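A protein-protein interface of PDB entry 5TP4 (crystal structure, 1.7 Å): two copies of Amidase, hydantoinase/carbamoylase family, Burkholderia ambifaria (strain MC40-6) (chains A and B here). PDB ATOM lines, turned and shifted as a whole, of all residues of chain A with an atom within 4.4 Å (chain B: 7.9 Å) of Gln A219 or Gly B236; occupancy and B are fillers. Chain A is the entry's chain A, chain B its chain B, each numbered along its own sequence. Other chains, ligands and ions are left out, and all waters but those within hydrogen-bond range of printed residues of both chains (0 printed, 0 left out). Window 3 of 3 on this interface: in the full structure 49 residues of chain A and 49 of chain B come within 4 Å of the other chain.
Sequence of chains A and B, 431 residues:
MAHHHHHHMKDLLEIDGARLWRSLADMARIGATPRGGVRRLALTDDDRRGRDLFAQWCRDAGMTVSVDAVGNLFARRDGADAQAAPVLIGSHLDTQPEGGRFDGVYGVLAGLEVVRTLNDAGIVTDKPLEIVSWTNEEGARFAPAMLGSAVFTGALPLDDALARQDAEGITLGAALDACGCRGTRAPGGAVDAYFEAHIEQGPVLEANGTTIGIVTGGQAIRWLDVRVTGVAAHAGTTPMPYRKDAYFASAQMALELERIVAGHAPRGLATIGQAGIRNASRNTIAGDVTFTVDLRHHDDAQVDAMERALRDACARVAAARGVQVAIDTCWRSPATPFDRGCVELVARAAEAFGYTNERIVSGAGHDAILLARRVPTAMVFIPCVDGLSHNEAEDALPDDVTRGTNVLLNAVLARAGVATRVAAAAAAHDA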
ATOM      1  N   GLY A 218       3.660 -32.644   6.271  1.00  0.00           N
ATOM      2  CA  GLY A 218       2.923 -31.460   5.864  1.00  0.00           C
ATOM      3  C   GLY A 218       3.145 -30.316   6.839  1.00  0.00           C
ATOM      4  O   GLY A 218       3.506 -30.550   7.992  1.00  0.00           O
ATOM      5  N   GLN A 219       2.937 -29.079   6.374  1.00  0.00           N
ATOM      6  CA  GLN A 219       3.127 -27.868   7.166  1.00  0.00           C
ATOM      7  C   GLN A 219       1.986 -27.656   8.160  1.00  0.00           C
ATOM      8  O   GLN A 219       0.873 -28.154   7.991  1.00  0.00           O
ATOM      9  CB  GLN A 219       3.178 -26.633   6.256  1.00  0.00           C
ATOM     10  CG  GLN A 219       4.309 -26.647   5.258  1.00  0.00           C
ATOM     11  CD  GLN A 219       3.985 -25.852   4.010  1.00  0.00           C
ATOM     12  OE1 GLN A 219       2.867 -25.938   3.474  1.00  0.00           O
ATOM     13  NE2 GLN A 219       4.957 -25.076   3.525  1.00  0.00           N
ATOM     14  N   ALA A 220       2.277 -26.856   9.175  1.00  0.00           N
ATOM     15  CA  ALA A 220       1.246 -26.201   9.981  1.00  0.00           C
ATOM     16  C   ALA A 220       0.780 -24.971   9.209  1.00  0.00           C
ATOM     17  O   ALA A 220       1.614 -24.225   8.690  1.00  0.00           O
ATOM     18  CB  ALA A 220       1.820 -25.782  11.330  1.00  0.00           C
ATOM     19  N   ILE A 221      -0.536 -24.781   9.096  1.00  0.00           N
ATOM     20  CA  ILE A 221      -1.117 -23.746   8.238  1.00  0.00           C
ATOM     21  C   ILE A 221      -2.115 -22.924   9.040  1.00  0.00           C
ATOM     22  O   ILE A 221      -2.907 -23.481   9.804  1.00  0.00           O
ATOM     23  CB  ILE A 221      -1.831 -24.356   7.010  1.00  0.00           C
ATOM     24  CG1 ILE A 221      -0.920 -25.358   6.282  1.00  0.00           C
ATOM     25  CG2 ILE A 221      -2.331 -23.234   6.057  1.00  0.00           C
ATOM     26  CD1 ILE A 221      -1.661 -26.165   5.247  1.00  0.00           C
ATOM     27  N   LEU A 269       6.460 -19.245   5.845  1.00  0.00           N
ATOM     28  CA  LEU A 269       5.970 -18.667   4.602  1.00  0.00           C
ATOM     29  C   LEU A 269       4.743 -17.818   4.900  1.00  0.00           C
ATOM     30  O   LEU A 269       4.000 -18.094   5.847  1.00  0.00           O
ATOM     31  CB  LEU A 269       5.583 -19.755   3.589  1.00  0.00           C
ATOM     32  CG  LEU A 269       6.590 -20.878   3.286  1.00  0.00           C
ATOM     33  CD1 LEU A 269       5.880 -21.909   2.399  1.00  0.00           C
ATOM     34  CD2 LEU A 269       7.783 -20.277   2.543  1.00  0.00           C
ATOM     35  N   ARG A 296       2.408 -20.289   6.996  1.00  0.00           N
ATOM     36  CA  ARG A 296       2.897 -21.664   7.052  1.00  0.00           C
ATOM     37  C   ARG A 296       4.192 -21.741   7.836  1.00  0.00           C
ATOM     38  O   ARG A 296       4.991 -20.806   7.840  1.00  0.00           O
ATOM     39  CB  ARG A 296       3.175 -22.230   5.665  1.00  0.00           C
ATOM     40  CG  ARG A 296       2.083 -21.877   4.689  1.00  0.00           C
ATOM     41  CD  ARG A 296       1.590 -23.055   3.938  1.00  0.00           C
ATOM     42  NE  ARG A 296       0.374 -22.732   3.190  1.00  0.00           N
ATOM     43  CZ  ARG A 296      -0.318 -23.630   2.496  1.00  0.00           C
ATOM     44  NH1 ARG A 296       0.098 -24.892   2.457  1.00  0.00           N
ATOM     45  NH2 ARG A 296      -1.433 -23.276   1.871  1.00  0.00           N
ATOM     46  N   HIS A 297       4.386 -22.884   8.495  1.00  0.00           N
ATOM     47  CA  HIS A 297       5.676 -23.220   9.073  1.00  0.00           C
ATOM     48  C   HIS A 297       5.738 -24.735   9.176  1.00  0.00           C
ATOM     49  O   HIS A 297       4.766 -25.429   8.878  1.00  0.00           O
ATOM     50  CB  HIS A 297       5.874 -22.547  10.435  1.00  0.00           C
ATOM     51  CG  HIS A 297       7.308 -22.340  10.803  1.00  0.00           C
ATOM     52  ND1 HIS A 297       8.111 -23.365  11.256  1.00  0.00           N
ATOM     53  CD2 HIS A 297       8.069 -21.217  10.839  1.00  0.00           C
ATOM     54  CE1 HIS A 297       9.311 -22.887  11.536  1.00  0.00           C
ATOM     55  NE2 HIS A 297       9.313 -21.588  11.293  1.00  0.00           N
ATOM     56  N   SER A 333      -4.705 -25.775  10.350  1.00  0.00           N
ATOM     57  CA  SER A 333      -4.420 -27.166  10.113  1.00  0.00           C
ATOM     58  C   SER A 333      -3.083 -27.459  10.770  1.00  0.00           C
ATOM     59  O   SER A 333      -2.146 -26.661  10.649  1.00  0.00           O
ATOM     60  CB  SER A 333      -4.360 -27.480   8.619  1.00  0.00           C
ATOM     61  OG  SER A 333      -4.735 -28.830   8.402  1.00  0.00           O
ATOM     62  N   PRO A 334      -2.962 -28.586  11.461  1.00  0.00           N
ATOM     63  CA  PRO A 334      -1.736 -28.872  12.200  1.00  0.00           C
ATOM     64  C   PRO A 334      -0.656 -29.424  11.287  1.00  0.00           C
ATOM     65  O   PRO A 334      -0.924 -29.980  10.216  1.00  0.00           O
ATOM     66  CB  PRO A 334      -2.182 -29.939  13.212  1.00  0.00           C
ATOM     67  CG  PRO A 334      -3.236 -30.704  12.440  1.00  0.00           C
ATOM     68  CD  PRO A 334      -3.974 -29.649  11.629  1.00  0.00           C
ATOM     69  N   ALA A 335       0.579 -29.279  11.737  1.00  0.00           N
ATOM     70  CA  ALA A 335       1.657 -29.945  11.018  1.00  0.00           C
ATOM     71  C   ALA A 335       1.413 -31.439  11.057  1.00  0.00           C
ATOM     72  O   ALA A 335       0.882 -31.974  12.031  1.00  0.00           O
ATOM     73  CB  ALA A 335       3.016 -29.646  11.643  1.00  0.00           C
ATOM     74  N   VAL A 361       9.426 -30.556   2.595  1.00  0.00           N
ATOM     75  CA  VAL A 361       8.081 -30.609   3.152  1.00  0.00           C
ATOM     76  C   VAL A 361       7.082 -30.587   2.004  1.00  0.00           C
ATOM     77  O   VAL A 361       7.320 -29.988   0.954  1.00  0.00           O
ATOM     78  CB  VAL A 361       7.844 -29.440   4.149  1.00  0.00           C
ATOM     79  CG1 VAL A 361       7.632 -28.118   3.407  1.00  0.00           C
ATOM     80  CG2 VAL A 361       6.673 -29.737   5.112  1.00  0.00           C
ATOM     81  N   SER A 362       5.954 -31.268   2.185  1.00  0.00           N
ATOM     82  CA  SER A 362       4.879 -31.090   1.226  1.00  0.00           C
ATOM     83  C   SER A 362       4.216 -29.738   1.451  1.00  0.00           C
ATOM     84  O   SER A 362       3.691 -29.481   2.542  1.00  0.00           O
ATOM     85  CB  SER A 362       3.852 -32.208   1.342  1.00  0.00           C
ATOM     86  OG  SER A 362       2.896 -32.028   0.331  1.00  0.00           O
ATOM     87  N   GLY A 363       4.247 -28.872   0.414  1.00  0.00           N
ATOM     88  CA  GLY A 363       3.617 -27.562   0.490  1.00  0.00           C
ATOM     89  C   GLY A 363       2.142 -27.561   0.230  1.00  0.00           C
ATOM     90  O   GLY A 363       1.488 -26.520   0.358  1.00  0.00           O
ATOM     91  N   ALA B 233       1.911 -18.429  -7.932  1.00  0.00           N
ATOM     92  CA  ALA B 233       2.414 -19.735  -7.550  1.00  0.00           C
ATOM     93  C   ALA B 233       1.781 -20.140  -6.224  1.00  0.00           C
ATOM     94  O   ALA B 233       1.193 -19.320  -5.517  1.00  0.00           O
ATOM     95  CB  ALA B 233       3.946 -19.694  -7.461  1.00  0.00           C
ATOM     96  N   HIS B 234       1.887 -21.417  -5.895  1.00  0.00           N
ATOM     97  CA  HIS B 234       1.200 -21.917  -4.710  1.00  0.00           C
ATOM     98  C   HIS B 234       1.827 -21.379  -3.415  1.00  0.00           C
ATOM     99  O   HIS B 234       3.053 -21.377  -3.245  1.00  0.00           O
ATOM    100  CB  HIS B 234       1.226 -23.445  -4.738  1.00  0.00           C
ATOM    101  CG  HIS B 234       0.322 -24.094  -3.738  1.00  0.00           C
ATOM    102  ND1 HIS B 234       0.668 -24.250  -2.415  1.00  0.00           N
ATOM    103  CD2 HIS B 234      -0.886 -24.691  -3.884  1.00  0.00           C
ATOM    104  CE1 HIS B 234      -0.297 -24.883  -1.779  1.00  0.00           C
ATOM    105  NE2 HIS B 234      -1.254 -25.166  -2.646  1.00  0.00           N
ATOM    106  N   ALA B 235       0.958 -20.952  -2.482  1.00  0.00           N
ATOM    107  CA  ALA B 235       1.365 -20.323  -1.220  1.00  0.00           C
ATOM    108  C   ALA B 235       2.123 -21.253  -0.286  1.00  0.00           C
ATOM    109  O   ALA B 235       2.804 -20.769   0.628  1.00  0.00           O
ATOM    110  CB  ALA B 235       0.144 -19.792  -0.459  1.00  0.00           C
ATOM    111  N   GLY B 236       2.009 -22.562  -0.466  1.00  0.00           N
ATOM    112  CA  GLY B 236       2.683 -23.492   0.428  1.00  0.00           C
ATOM    113  C   GLY B 236       3.888 -24.177  -0.195  1.00  0.00           C
ATOM    114  O   GLY B 236       4.834 -24.516   0.515  1.00  0.00           O
ATOM    115  N   THR B 237       3.871 -24.403  -1.510  1.00  0.00           N
ATOM    116  CA  THR B 237       4.954 -25.140  -2.169  1.00  0.00           C
ATOM    117  C   THR B 237       6.101 -24.244  -2.631  1.00  0.00           C
ATOM    118  O   THR B 237       7.114 -24.764  -3.113  1.00  0.00           O
ATOM    119  CB  THR B 237       4.447 -25.882  -3.414  1.00  0.00           C
ATOM    120  OG1 THR B 237       4.113 -24.899  -4.398  1.00  0.00           O
ATOM    121  CG2 THR B 237       3.218 -26.733  -3.110  1.00  0.00           C
ATOM    122  N   THR B 238       5.957 -22.922  -2.536  1.00  0.00           N
ATOM    123  CA  THR B 238       6.919 -21.990  -3.120  1.00  0.00           C
ATOM    124  C   THR B 238       7.710 -21.284  -2.034  1.00  0.00           C
ATOM    125  O   THR B 238       7.179 -20.381  -1.378  1.00  0.00           O
ATOM    126  CB  THR B 238       6.191 -20.956  -3.974  1.00  0.00           C
ATOM    127  OG1 THR B 238       5.303 -21.606  -4.888  1.00  0.00           O
ATOM    128  CG2 THR B 238       7.200 -20.084  -4.752  1.00  0.00           C
ATOM    129  N   PRO B 239       8.966 -21.635  -1.796  1.00  0.00           N
ATOM    130  CA  PRO B 239       9.724 -20.921  -0.765  1.00  0.00           C
ATOM    131  C   PRO B 239       9.885 -19.450  -1.125  1.00  0.00           C
ATOM    132  O   PRO B 239       9.761 -19.039  -2.287  1.00  0.00           O
ATOM    133  CB  PRO B 239      11.077 -21.644  -0.734  1.00  0.00           C
ATOM    134  CG  PRO B 239      10.764 -23.029  -1.236  1.00  0.00           C
ATOM    135  CD  PRO B 239       9.695 -22.822  -2.294  1.00  0.00           C
ATOM    136  N   ARG B 243       9.777 -16.368  -5.031  1.00  0.00           N
ATOM    137  CA  ARG B 243       8.516 -15.698  -5.268  1.00  0.00           C
ATOM    138  C   ARG B 243       8.692 -14.389  -6.022  1.00  0.00           C
ATOM    139  O   ARG B 243       9.701 -13.692  -5.888  1.00  0.00           O
ATOM    140  CB  ARG B 243       7.820 -15.422  -3.940  1.00  0.00           C
ATOM    141  CG  ARG B 243       7.521 -16.684  -3.199  1.00  0.00           C
ATOM    142  CD  ARG B 243       6.722 -16.408  -1.971  1.00  0.00           C
ATOM    143  NE  ARG B 243       6.308 -17.700  -1.389  1.00  0.00           N
ATOM    144  CZ  ARG B 243       5.239 -17.878  -0.645  1.00  0.00           C
ATOM    145  NH1 ARG B 243       4.438 -16.847  -0.368  1.00  0.00           N
ATOM    146  NH2 ARG B 243       4.967 -19.105  -0.201  1.00  0.00           N
ATOM    147  N   ARG B 282      -6.896 -17.734  -1.664  1.00  0.00           N
ATOM    148  CA  ARG B 282      -6.159 -17.566  -0.413  1.00  0.00           C
ATOM    149  C   ARG B 282      -4.800 -18.246  -0.434  1.00  0.00           C
ATOM    150  O   ARG B 282      -3.864 -17.783   0.233  1.00  0.00           O
ATOM    151  CB  ARG B 282      -6.961 -18.135   0.754  1.00  0.00           C
ATOM    152  CG  ARG B 282      -8.238 -17.402   1.051  1.00  0.00           C
ATOM    153  CD  ARG B 282      -9.026 -18.203   2.075  1.00  0.00           C
ATOM    154  NE  ARG B 282     -10.173 -17.455   2.555  1.00  0.00           N
ATOM    155  CZ  ARG B 282     -10.148 -16.661   3.617  1.00  0.00           C
ATOM    156  NH1 ARG B 282      -9.022 -16.512   4.309  1.00  0.00           N
ATOM    157  NH2 ARG B 282     -11.249 -16.009   3.975  1.00  0.00           N
ATOM    158  N   ASN B 283      -4.668 -19.366  -1.144  1.00  0.00           N
ATOM    159  CA  ASN B 283      -3.412 -20.105  -1.118  1.00  0.00           C
ATOM    160  C   ASN B 283      -2.637 -19.967  -2.428  1.00  0.00           C
ATOM    161  O   ASN B 283      -1.859 -20.853  -2.794  1.00  0.00           O
ATOM    162  CB  ASN B 283      -3.646 -21.575  -0.777  1.00  0.00           C
ATOM    163  CG  ASN B 283      -4.558 -22.274  -1.755  1.00  0.00           C
ATOM    164  OD1 ASN B 283      -5.217 -21.633  -2.592  1.00  0.00           O
ATOM    165  ND2 ASN B 283      -4.605 -23.612  -1.652  1.00  0.00           N
ATOM    166  N   THR B 284      -2.820 -18.849  -3.116  1.00  0.00           N
ATOM    167  CA  THR B 284      -2.063 -18.548  -4.323  1.00  0.00           C
ATOM    168  C   THR B 284      -1.427 -17.174  -4.193  1.00  0.00           C
ATOM    169  O   THR B 284      -2.113 -16.193  -3.883  1.00  0.00           O
ATOM    170  CB  THR B 284      -2.967 -18.609  -5.552  1.00  0.00           C
ATOM    171  OG1 THR B 284      -3.628 -19.885  -5.573  1.00  0.00           O
ATOM    172  CG2 THR B 284      -2.134 -18.495  -6.819  1.00  0.00           C
ATOM    173  N   ILE B 285      -0.111 -17.114  -4.432  1.00  0.00           N
ATOM    174  CA  ILE B 285       0.582 -15.831  -4.524  1.00  0.00           C
ATOM    175  C   ILE B 285      -0.069 -14.945  -5.580  1.00  0.00           C
ATOM    176  O   ILE B 285      -0.448 -15.405  -6.666  1.00  0.00           O
ATOM    177  CB  ILE B 285       2.065 -16.090  -4.843  1.00  0.00           C
ATOM    178  CG1 ILE B 285       2.694 -16.900  -3.699  1.00  0.00           C
ATOM    179  CG2 ILE B 285       2.836 -14.759  -5.157  1.00  0.00           C
ATOM    180  CD1 ILE B 285       3.944 -17.665  -4.117  1.00  0.00           C
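The side-chain amide nitrogen (NE2) of Gln A219 lies within hydrogen-bond range of the backbone carbonyl oxygen (O) of Gly B236 (3.1 Å).
The guanidinium group (NH1) of Arg A296 sits at hydrogen-bond distance from the side-chain amide oxygen (OE1) of Gln A219 (3.1 Å).
The backbone carbonyl oxygen (O) of Gly A363 is in hydrogen-bond range of the guanidinium group (NH1) of Arg A296, 3.0 Å away.
ND1 of His B234 sits at hydrogen-bond distance from N of Gly B236, 2.9 Å away.
ND1 of His B234 lies within hydrogen-bond range of N of Thr B237, 3.3 Å away.
OG1 of Thr B238 is in hydrogen-bond range of O of His B234 (2.8 Å).
The guanidinium group (NH2) of Arg B243 lies within hydrogen-bond range of the backbone carbonyl oxygen (O) of Thr B238, at 2.8 Å.
CD1 of Leu A269 touches O of Ala B235, 3.7 Å away.
Gly B236 touches Leu A269 (O to CD1, 3.4 Å).
CD2 of Leu A269 touches O of Thr B238 (3.97 Å).
Leu A269 touches Pro B239.
Leu A269 touches Arg B243 (CB to NH2, 3.9 Å).
Arg A296 touches Gly B236 (NH1 to CA, 3.6 Å).
Arg A296 touches Asn B283 (NH2 to CB, 3.8 Å).
Gly A363 touches His B234.
O of Gly A363 touches CA of Gly B236 (3.3 Å).
CG2 of Thr B237 touches C of Gly A363, 3.6 Å away.
Of chain B, only Gly B236 comes within 4 Å of Gln A219.
Gly B236 touches just these residues of chain A: Gln A219, Leu A269, Arg A296 and Gly A363.
Of the printed residues of chain A, Arg B243 touches Leu A269 (3.9 Å).
Printed residues of chain B within 4 Å of Leu A269: Ala B235, Gly B236, Thr B238, Pro B239 and Arg B243.
Of the printed residues of chain A, His B234 touches Gly A363.
Printed residues of chain A within 4 Å of Pro B239: Leu A269 (3.9 Å).
Pro A334 touches none of the printed residues of chain B.
The nearest residue of chain B that does not touch Gln A219 is Thr B237 (5.2 Å).
Of the 13 printed residues of chain A, 4 touch a printed residue of chain B.
Printed residues of chain A that touch a printed residue of chain B: Gln A219, Leu A269, Arg A296 and Gly A363.
Hydrophobic or aromatic side chains of chain A that line the printed part of chain B: Leu A269.
Of the 12 printed residues of chain B, 8 touch a printed residue of chain A.
Printed residues of chain B that touch a printed residue of chain A: His B234, Ala B235, Gly B236, Thr B237, Thr B238, Pro B239, Arg B243 and Asn B283.
Hydrophobic or aromatic side chains of chain B that line the printed part of chain A: His B234.
Among the printed residues, no Asp or Glu carboxylate lies within 4 Å of a Lys or Arg side-chain nitrogen of the other chain.
No position is printed for both chains.
Of the 11 pairs that touch across the chains among the printed residues, none has its exchanged pair printed and touching as well.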
